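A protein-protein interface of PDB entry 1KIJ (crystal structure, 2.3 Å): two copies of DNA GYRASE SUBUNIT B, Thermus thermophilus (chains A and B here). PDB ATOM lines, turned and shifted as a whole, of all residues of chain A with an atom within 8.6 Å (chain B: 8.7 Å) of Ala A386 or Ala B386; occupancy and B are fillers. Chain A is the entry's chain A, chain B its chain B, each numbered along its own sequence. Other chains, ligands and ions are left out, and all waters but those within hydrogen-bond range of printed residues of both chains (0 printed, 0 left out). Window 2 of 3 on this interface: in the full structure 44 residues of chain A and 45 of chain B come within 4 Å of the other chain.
CB of Ala A379 touches CG of Arg B387 (3.9 Å). Ala A383 touches Ala B383 (CB to CB, 3.7 Å). O of Ala B382 touches CB of Ala A386, 3.9 Å away. Ala A386 touches Ala B386. Arg A387 touches Ala B379. CA of Arg B380 touches NH2 of Arg A387, at 3.6 Å. NE of Arg A387 touches CB of Ala B383, 3.5 Å away.
Ala B386 touches one residue of chain A. Of the printed residues of chain A, Ala B383 touches Ala A383 and Arg A387. Of the printed residues of chain B, Ala A379 touches Arg B387 (3.9 Å). Arg B384 touches none of the printed residues of chain A. The nearest residue of chain B that does not touch Ala A386 is Ala B383 (4.2 Å). The nearest printed residue of chain B that does not touch Ala A379 is Val B390 (4.1 Å).
Of the 13 printed residues of chain B, 6 touch a printed residue of chain A. Hydrophobic or aromatic side chains of chain B that line the printed part of chain A: Ala B383 and Ala B386. Along chain A the printed residues that touch a printed residue of chain B span positions 379 to 387. Among the printed residues, 7 pairs touch across the chains.
Ala A379 touches Arg B387, and with the chains exchanged Arg A387 touches Ala B379. Ala A386 touches Ala B382, but with the chains exchanged Ala A382 does not touch Ala B386 (4.1 Å). Ala A386 touches its own counterpart, Ala B386. Arg A387 touches Arg B380, but with the chains exchanged Arg A380 does not touch Arg B387 (4.9 Å). Positions printed for both chains: 378, 379, 380, 381, 382, 383, 384, 385, 386, 387, 388, 389 and 390.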
ATOM      1  N   GLN A 378     -18.815 -23.615  29.385  1.00  0.00           N
ATOM      2  CA  GLN A 378     -18.964 -23.940  27.973  1.00  0.00           C
ATOM      3  C   GLN A 378     -19.644 -22.802  27.228  1.00  0.00           C
ATOM      4  O   GLN A 378     -19.202 -22.411  26.161  1.00  0.00           O
ATOM      5  CB  GLN A 378     -19.765 -25.233  27.784  1.00  0.00           C
ATOM      6  CG  GLN A 378     -18.902 -26.488  27.678  1.00  0.00           C
ATOM      7  CD  GLN A 378     -19.593 -27.624  26.928  1.00  0.00           C
ATOM      8  OE1 GLN A 378     -19.014 -28.693  26.728  1.00  0.00           O
ATOM      9  NE2 GLN A 378     -20.835 -27.393  26.506  1.00  0.00           N
ATOM     10  N   ALA A 379     -20.724 -22.275  27.802  1.00  0.00           N
ATOM     11  CA  ALA A 379     -21.454 -21.168  27.189  1.00  0.00           C
ATOM     12  C   ALA A 379     -20.509 -19.997  26.911  1.00  0.00           C
ATOM     13  O   ALA A 379     -20.597 -19.346  25.882  1.00  0.00           O
ATOM     14  CB  ALA A 379     -22.586 -20.724  28.102  1.00  0.00           C
ATOM     15  N   ARG A 380     -19.609 -19.743  27.855  1.00  0.00           N
ATOM     16  CA  ARG A 380     -18.628 -18.671  27.732  1.00  0.00           C
ATOM     17  C   ARG A 380     -17.689 -18.926  26.552  1.00  0.00           C
ATOM     18  O   ARG A 380     -17.391 -18.021  25.782  1.00  0.00           O
ATOM     19  CB  ARG A 380     -17.817 -18.564  29.029  1.00  0.00           C
ATOM     20  CG  ARG A 380     -16.688 -17.552  28.989  1.00  0.00           C
ATOM     21  CD  ARG A 380     -16.001 -17.431  30.342  1.00  0.00           C
ATOM     22  NE  ARG A 380     -14.657 -18.010  30.358  1.00  0.00           N
ATOM     23  CZ  ARG A 380     -14.381 -19.308  30.483  1.00  0.00           C
ATOM     24  NH1 ARG A 380     -15.355 -20.201  30.608  1.00  0.00           N
ATOM     25  NH2 ARG A 380     -13.116 -19.713  30.484  1.00  0.00           N
ATOM     26  N   GLU A 381     -17.233 -20.168  26.417  1.00  0.00           N
ATOM     27  CA  GLU A 381     -16.322 -20.532  25.336  1.00  0.00           C
ATOM     28  C   GLU A 381     -17.036 -20.697  23.990  1.00  0.00           C
ATOM     29  O   GLU A 381     -16.413 -20.637  22.939  1.00  0.00           O
ATOM     30  CB  GLU A 381     -15.564 -21.810  25.706  1.00  0.00           C
ATOM     31  CG  GLU A 381     -14.374 -22.112  24.803  1.00  0.00           C
ATOM     32  CD  GLU A 381     -13.359 -20.974  24.740  1.00  0.00           C
ATOM     33  OE1 GLU A 381     -12.326 -21.143  24.055  1.00  0.00           O
ATOM     34  OE2 GLU A 381     -13.586 -19.915  25.367  1.00  0.00           O
ATOM     35  N   ALA A 382     -18.346 -20.906  24.037  1.00  0.00           N
ATOM     36  CA  ALA A 382     -19.145 -21.044  22.827  1.00  0.00           C
ATOM     37  C   ALA A 382     -19.288 -19.656  22.198  1.00  0.00           C
ATOM     38  O   ALA A 382     -19.245 -19.501  20.985  1.00  0.00           O
ATOM     39  CB  ALA A 382     -20.517 -21.615  23.170  1.00  0.00           C
ATOM     40  N   ALA A 383     -19.462 -18.647  23.045  1.00  0.00           N
ATOM     41  CA  ALA A 383     -19.589 -17.273  22.580  1.00  0.00           C
ATOM     42  C   ALA A 383     -18.236 -16.788  22.066  1.00  0.00           C
ATOM     43  O   ALA A 383     -18.176 -15.997  21.140  1.00  0.00           O
ATOM     44  CB  ALA A 383     -20.070 -16.375  23.715  1.00  0.00           C
ATOM     45  N   ARG A 384     -17.153 -17.259  22.678  1.00  0.00           N
ATOM     46  CA  ARG A 384     -15.827 -16.851  22.232  1.00  0.00           C
ATOM     47  C   ARG A 384     -15.660 -17.330  20.795  1.00  0.00           C
ATOM     48  O   ARG A 384     -15.405 -16.535  19.901  1.00  0.00           O
ATOM     49  CB  ARG A 384     -14.731 -17.460  23.115  1.00  0.00           C
ATOM     50  CG  ARG A 384     -13.393 -16.718  23.038  1.00  0.00           C
ATOM     51  CD  ARG A 384     -12.878 -16.609  21.599  1.00  0.00           C
ATOM     52  NE  ARG A 384     -11.823 -15.604  21.448  1.00  0.00           N
ATOM     53  CZ  ARG A 384     -10.568 -15.745  21.869  1.00  0.00           C
ATOM     54  NH1 ARG A 384     -10.174 -16.859  22.478  1.00  0.00           N
ATOM     55  NH2 ARG A 384      -9.700 -14.757  21.685  1.00  0.00           N
ATOM     56  N   LYS A 385     -15.813 -18.638  20.589  1.00  0.00           N
ATOM     57  CA  LYS A 385     -15.699 -19.235  19.263  1.00  0.00           C
ATOM     58  C   LYS A 385     -16.535 -18.467  18.248  1.00  0.00           C
ATOM     59  O   LYS A 385     -16.058 -18.118  17.176  1.00  0.00           O
ATOM     60  CB  LYS A 385     -16.162 -20.696  19.294  1.00  0.00           C
ATOM     61  CG  LYS A 385     -15.061 -21.716  19.580  1.00  0.00           C
ATOM     62  CD  LYS A 385     -15.631 -23.129  19.574  1.00  0.00           C
ATOM     63  CE  LYS A 385     -14.539 -24.197  19.592  1.00  0.00           C
ATOM     64  NZ  LYS A 385     -13.714 -24.209  18.343  1.00  0.00           N
ATOM     65  N   ALA A 386     -17.791 -18.210  18.604  1.00  0.00           N
ATOM     66  CA  ALA A 386     -18.711 -17.486  17.738  1.00  0.00           C
ATOM     67  C   ALA A 386     -18.157 -16.126  17.327  1.00  0.00           C
ATOM     68  O   ALA A 386     -18.179 -15.775  16.158  1.00  0.00           O
ATOM     69  CB  ALA A 386     -20.059 -17.312  18.442  1.00  0.00           C
ATOM     70  N   ARG A 387     -17.658 -15.368  18.298  1.00  0.00           N
ATOM     71  CA  ARG A 387     -17.115 -14.044  18.026  1.00  0.00           C
ATOM     72  C   ARG A 387     -15.815 -14.062  17.231  1.00  0.00           C
ATOM     73  O   ARG A 387     -15.626 -13.241  16.345  1.00  0.00           O
ATOM     74  CB  ARG A 387     -16.925 -13.272  19.334  1.00  0.00           C
ATOM     75  CG  ARG A 387     -18.236 -12.879  19.993  1.00  0.00           C
ATOM     76  CD  ARG A 387     -18.031 -11.821  21.059  1.00  0.00           C
ATOM     77  NE  ARG A 387     -19.306 -11.274  21.516  1.00  0.00           N
ATOM     78  CZ  ARG A 387     -19.433 -10.248  22.353  1.00  0.00           C
ATOM     79  NH1 ARG A 387     -18.356  -9.642  22.838  1.00  0.00           N
ATOM     80  NH2 ARG A 387     -20.641  -9.824  22.701  1.00  0.00           N
ATOM     81  N   GLU A 388     -14.919 -14.994  17.545  1.00  0.00           N
ATOM     82  CA  GLU A 388     -13.658 -15.088  16.812  1.00  0.00           C
ATOM     83  C   GLU A 388     -13.946 -15.471  15.360  1.00  0.00           C
ATOM     84  O   GLU A 388     -13.119 -15.270  14.481  1.00  0.00           O
ATOM     85  CB  GLU A 388     -12.726 -16.124  17.458  1.00  0.00           C
ATOM     86  CG  GLU A 388     -13.186 -17.570  17.348  1.00  0.00           C
ATOM     87  CD  GLU A 388     -12.244 -18.536  18.053  1.00  0.00           C
ATOM     88  OE1 GLU A 388     -11.033 -18.527  17.736  1.00  0.00           O
ATOM     89  OE2 GLU A 388     -12.713 -19.307  18.922  1.00  0.00           O
ATOM     90  N   LEU A 389     -15.132 -16.028  15.132  1.00  0.00           N
ATOM     91  CA  LEU A 389     -15.585 -16.433  13.811  1.00  0.00           C
ATOM     92  C   LEU A 389     -16.195 -15.221  13.103  1.00  0.00           C
ATOM     93  O   LEU A 389     -16.303 -15.195  11.882  1.00  0.00           O
ATOM     94  CB  LEU A 389     -16.620 -17.551  13.961  1.00  0.00           C
ATOM     95  CG  LEU A 389     -17.289 -18.187  12.741  1.00  0.00           C
ATOM     96  CD1 LEU A 389     -17.932 -19.504  13.163  1.00  0.00           C
ATOM     97  CD2 LEU A 389     -18.330 -17.242  12.145  1.00  0.00           C
ATOM     98  N   VAL A 390     -16.593 -14.227  13.893  1.00  0.00           N
ATOM     99  CA  VAL A 390     -17.182 -12.990  13.392  1.00  0.00           C
ATOM    100  C   VAL A 390     -18.459 -13.253  12.603  1.00  0.00           C
ATOM    101  O   VAL A 390     -19.562 -13.013  13.102  1.00  0.00           O
ATOM    102  CB  VAL A 390     -16.175 -12.211  12.503  1.00  0.00           C
ATOM    103  CG1 VAL A 390     -16.836 -10.973  11.923  1.00  0.00           C
ATOM    104  CG2 VAL A 390     -14.953 -11.815  13.323  1.00  0.00           C
ATOM    105  N   GLN B 378     -22.989  -7.338  15.142  1.00  0.00           N
ATOM    106  CA  GLN B 378     -23.075  -8.692  14.606  1.00  0.00           C
ATOM    107  C   GLN B 378     -22.425  -9.695  15.551  1.00  0.00           C
ATOM    108  O   GLN B 378     -23.010 -10.715  15.865  1.00  0.00           O
ATOM    109  CB  GLN B 378     -22.397  -8.756  13.239  1.00  0.00           C
ATOM    110  CG  GLN B 378     -23.175  -8.087  12.128  1.00  0.00           C
ATOM    111  CD  GLN B 378     -22.282  -7.657  10.984  1.00  0.00           C
ATOM    112  OE1 GLN B 378     -21.340  -8.358  10.616  1.00  0.00           O
ATOM    113  NE2 GLN B 378     -22.580  -6.497  10.406  1.00  0.00           N
ATOM    114  N   ALA B 379     -21.206  -9.397  15.994  1.00  0.00           N
ATOM    115  CA  ALA B 379     -20.495 -10.279  16.915  1.00  0.00           C
ATOM    116  C   ALA B 379     -21.345 -10.515  18.164  1.00  0.00           C
ATOM    117  O   ALA B 379     -21.431 -11.632  18.664  1.00  0.00           O
ATOM    118  CB  ALA B 379     -19.153  -9.664  17.299  1.00  0.00           C
ATOM    119  N   ARG B 380     -21.968  -9.451  18.662  1.00  0.00           N
ATOM    120  CA  ARG B 380     -22.825  -9.541  19.838  1.00  0.00           C
ATOM    121  C   ARG B 380     -23.971 -10.516  19.570  1.00  0.00           C
ATOM    122  O   ARG B 380     -24.286 -11.370  20.397  1.00  0.00           O
ATOM    123  CB  ARG B 380     -23.390  -8.157  20.180  1.00  0.00           C
ATOM    124  CG  ARG B 380     -24.470  -8.161  21.254  1.00  0.00           C
ATOM    125  CD  ARG B 380     -24.880  -6.742  21.632  1.00  0.00           C
ATOM    126  NE  ARG B 380     -25.360  -5.964  20.488  1.00  0.00           N
ATOM    127  CZ  ARG B 380     -26.528  -6.151  19.878  1.00  0.00           C
ATOM    128  NH1 ARG B 380     -27.361  -7.098  20.292  1.00  0.00           N
ATOM    129  NH2 ARG B 380     -26.866  -5.387  18.849  1.00  0.00           N
ATOM    130  N   GLU B 381     -24.583 -10.372  18.399  1.00  0.00           N
ATOM    131  CA  GLU B 381     -25.694 -11.215  17.975  1.00  0.00           C
ATOM    132  C   GLU B 381     -25.290 -12.692  17.944  1.00  0.00           C
ATOM    133  O   GLU B 381     -25.970 -13.539  18.516  1.00  0.00           O
ATOM    134  CB  GLU B 381     -26.170 -10.772  16.585  1.00  0.00           C
ATOM    135  CG  GLU B 381     -26.540  -9.289  16.510  1.00  0.00           C
ATOM    136  CD  GLU B 381     -26.865  -8.814  15.098  1.00  0.00           C
ATOM    137  OE1 GLU B 381     -27.062  -7.592  14.916  1.00  0.00           O
ATOM    138  OE2 GLU B 381     -26.924  -9.656  14.173  1.00  0.00           O
ATOM    139  N   ALA B 382     -24.175 -12.980  17.276  1.00  0.00           N
ATOM    140  CA  ALA B 382     -23.660 -14.339  17.148  1.00  0.00           C
ATOM    141  C   ALA B 382     -23.403 -15.011  18.495  1.00  0.00           C
ATOM    142  O   ALA B 382     -23.747 -16.168  18.686  1.00  0.00           O
ATOM    143  CB  ALA B 382     -22.384 -14.326  16.321  1.00  0.00           C
ATOM    144  N   ALA B 383     -22.791 -14.283  19.423  1.00  0.00           N
ATOM    145  CA  ALA B 383     -22.497 -14.824  20.750  1.00  0.00           C
ATOM    146  C   ALA B 383     -23.775 -15.060  21.551  1.00  0.00           C
ATOM    147  O   ALA B 383     -23.846 -15.974  22.364  1.00  0.00           O
ATOM    148  CB  ALA B 383     -21.578 -13.875  21.506  1.00  0.00           C
ATOM    149  N   ARG B 384     -24.779 -14.219  21.312  1.00  0.00           N
ATOM    150  CA  ARG B 384     -26.065 -14.323  21.994  1.00  0.00           C
ATOM    151  C   ARG B 384     -26.756 -15.637  21.630  1.00  0.00           C
ATOM    152  O   ARG B 384     -27.039 -16.462  22.488  1.00  0.00           O
ATOM    153  CB  ARG B 384     -26.951 -13.139  21.602  1.00  0.00           C
ATOM    154  CG  ARG B 384     -28.298 -13.085  22.307  1.00  0.00           C
ATOM    155  CD  ARG B 384     -29.066 -11.823  21.924  1.00  0.00           C
ATOM    156  NE  ARG B 384     -30.188 -12.080  21.021  1.00  0.00           N
ATOM    157  CZ  ARG B 384     -30.084 -12.390  19.730  1.00  0.00           C
ATOM    158  NH1 ARG B 384     -28.894 -12.491  19.146  1.00  0.00           N
ATOM    159  NH2 ARG B 384     -31.183 -12.599  19.015  1.00  0.00           N
ATOM    160  N   LYS B 385     -27.022 -15.821  20.342  1.00  0.00           N
ATOM    161  CA  LYS B 385     -27.667 -17.035  19.864  1.00  0.00           C
ATOM    162  C   LYS B 385     -26.876 -18.279  20.284  1.00  0.00           C
ATOM    163  O   LYS B 385     -27.448 -19.254  20.769  1.00  0.00           O
ATOM    164  CB  LYS B 385     -27.795 -16.979  18.341  1.00  0.00           C
ATOM    165  CG  LYS B 385     -28.594 -15.782  17.845  1.00  0.00           C
ATOM    166  CD  LYS B 385     -28.613 -15.700  16.325  1.00  0.00           C
ATOM    167  CE  LYS B 385     -29.422 -14.505  15.851  1.00  0.00           C
ATOM    168  NZ  LYS B 385     -30.835 -14.572  16.325  1.00  0.00           N
ATOM    169  N   ALA B 386     -25.560 -18.230  20.101  1.00  0.00           N
ATOM    170  CA  ALA B 386     -24.681 -19.341  20.453  1.00  0.00           C
ATOM    171  C   ALA B 386     -24.803 -19.723  21.926  1.00  0.00           C
ATOM    172  O   ALA B 386     -24.857 -20.898  22.275  1.00  0.00           O
ATOM    173  CB  ALA B 386     -23.231 -18.978  20.131  1.00  0.00           C
ATOM    174  N   ARG B 387     -24.838 -18.714  22.786  1.00  0.00           N
ATOM    175  CA  ARG B 387     -24.946 -18.931  24.220  1.00  0.00           C
ATOM    176  C   ARG B 387     -26.360 -19.361  24.595  1.00  0.00           C
ATOM    177  O   ARG B 387     -26.558 -20.096  25.560  1.00  0.00           O
ATOM    178  CB  ARG B 387     -24.554 -17.647  24.951  1.00  0.00           C
ATOM    179  CG  ARG B 387     -24.515 -17.742  26.464  1.00  0.00           C
ATOM    180  CD  ARG B 387     -23.488 -16.767  27.024  1.00  0.00           C
ATOM    181  NE  ARG B 387     -23.577 -15.454  26.387  1.00  0.00           N
ATOM    182  CZ  ARG B 387     -22.644 -14.512  26.473  1.00  0.00           C
ATOM    183  NH1 ARG B 387     -21.535 -14.723  27.176  1.00  0.00           N
ATOM    184  NH2 ARG B 387     -22.811 -13.359  25.835  1.00  0.00           N
ATOM    185  N   GLU B 388     -27.337 -18.907  23.814  1.00  0.00           N
ATOM    186  CA  GLU B 388     -28.740 -19.239  24.046  1.00  0.00           C
ATOM    187  C   GLU B 388     -29.110 -20.508  23.276  1.00  0.00           C
ATOM    188  O   GLU B 388     -30.280 -20.760  22.995  1.00  0.00           O
ATOM    189  CB  GLU B 388     -29.632 -18.081  23.587  1.00  0.00           C
ATOM    190  CG  GLU B 388     -31.023 -18.071  24.207  1.00  0.00           C
ATOM    191  CD  GLU B 388     -31.018 -17.621  25.661  1.00  0.00           C
ATOM    192  OE1 GLU B 388     -30.298 -18.233  26.483  1.00  0.00           O
ATOM    193  OE2 GLU B 388     -31.742 -16.650  25.983  1.00  0.00           O
ATOM    194  N   LEU B 389     -28.099 -21.299  22.934  1.00  0.00           N
ATOM    195  CA  LEU B 389     -28.299 -22.538  22.196  1.00  0.00           C
ATOM    196  C   LEU B 389     -28.040 -23.721  23.125  1.00  0.00           C
ATOM    197  O   LEU B 389     -28.702 -24.744  23.037  1.00  0.00           O
ATOM    198  CB  LEU B 389     -27.350 -22.583  20.995  1.00  0.00           C
ATOM    199  CG  LEU B 389     -27.645 -23.558  19.851  1.00  0.00           C
ATOM    200  CD1 LEU B 389     -29.015 -23.269  19.248  1.00  0.00           C
ATOM    201  CD2 LEU B 389     -26.569 -23.416  18.789  1.00  0.00           C
ATOM    202  N   VAL B 390     -27.072 -23.561  24.022  1.00  0.00           N
ATOM    203  CA  VAL B 390     -26.732 -24.606  24.981  1.00  0.00           C
ATOM    204  C   VAL B 390     -27.427 -24.342  26.319  1.00  0.00           C
ATOM    205  O   VAL B 390     -28.140 -25.251  26.798  1.00  0.00           O
ATOM    206  CB  VAL B 390     -25.198 -24.692  25.207  1.00  0.00           C
ATOM    207  CG1 VAL B 390     -24.664 -23.375  25.752  1.00  0.00           C
ATOM    208  CG2 VAL B 390     -24.878 -25.838  26.160  1.00  0.00           C
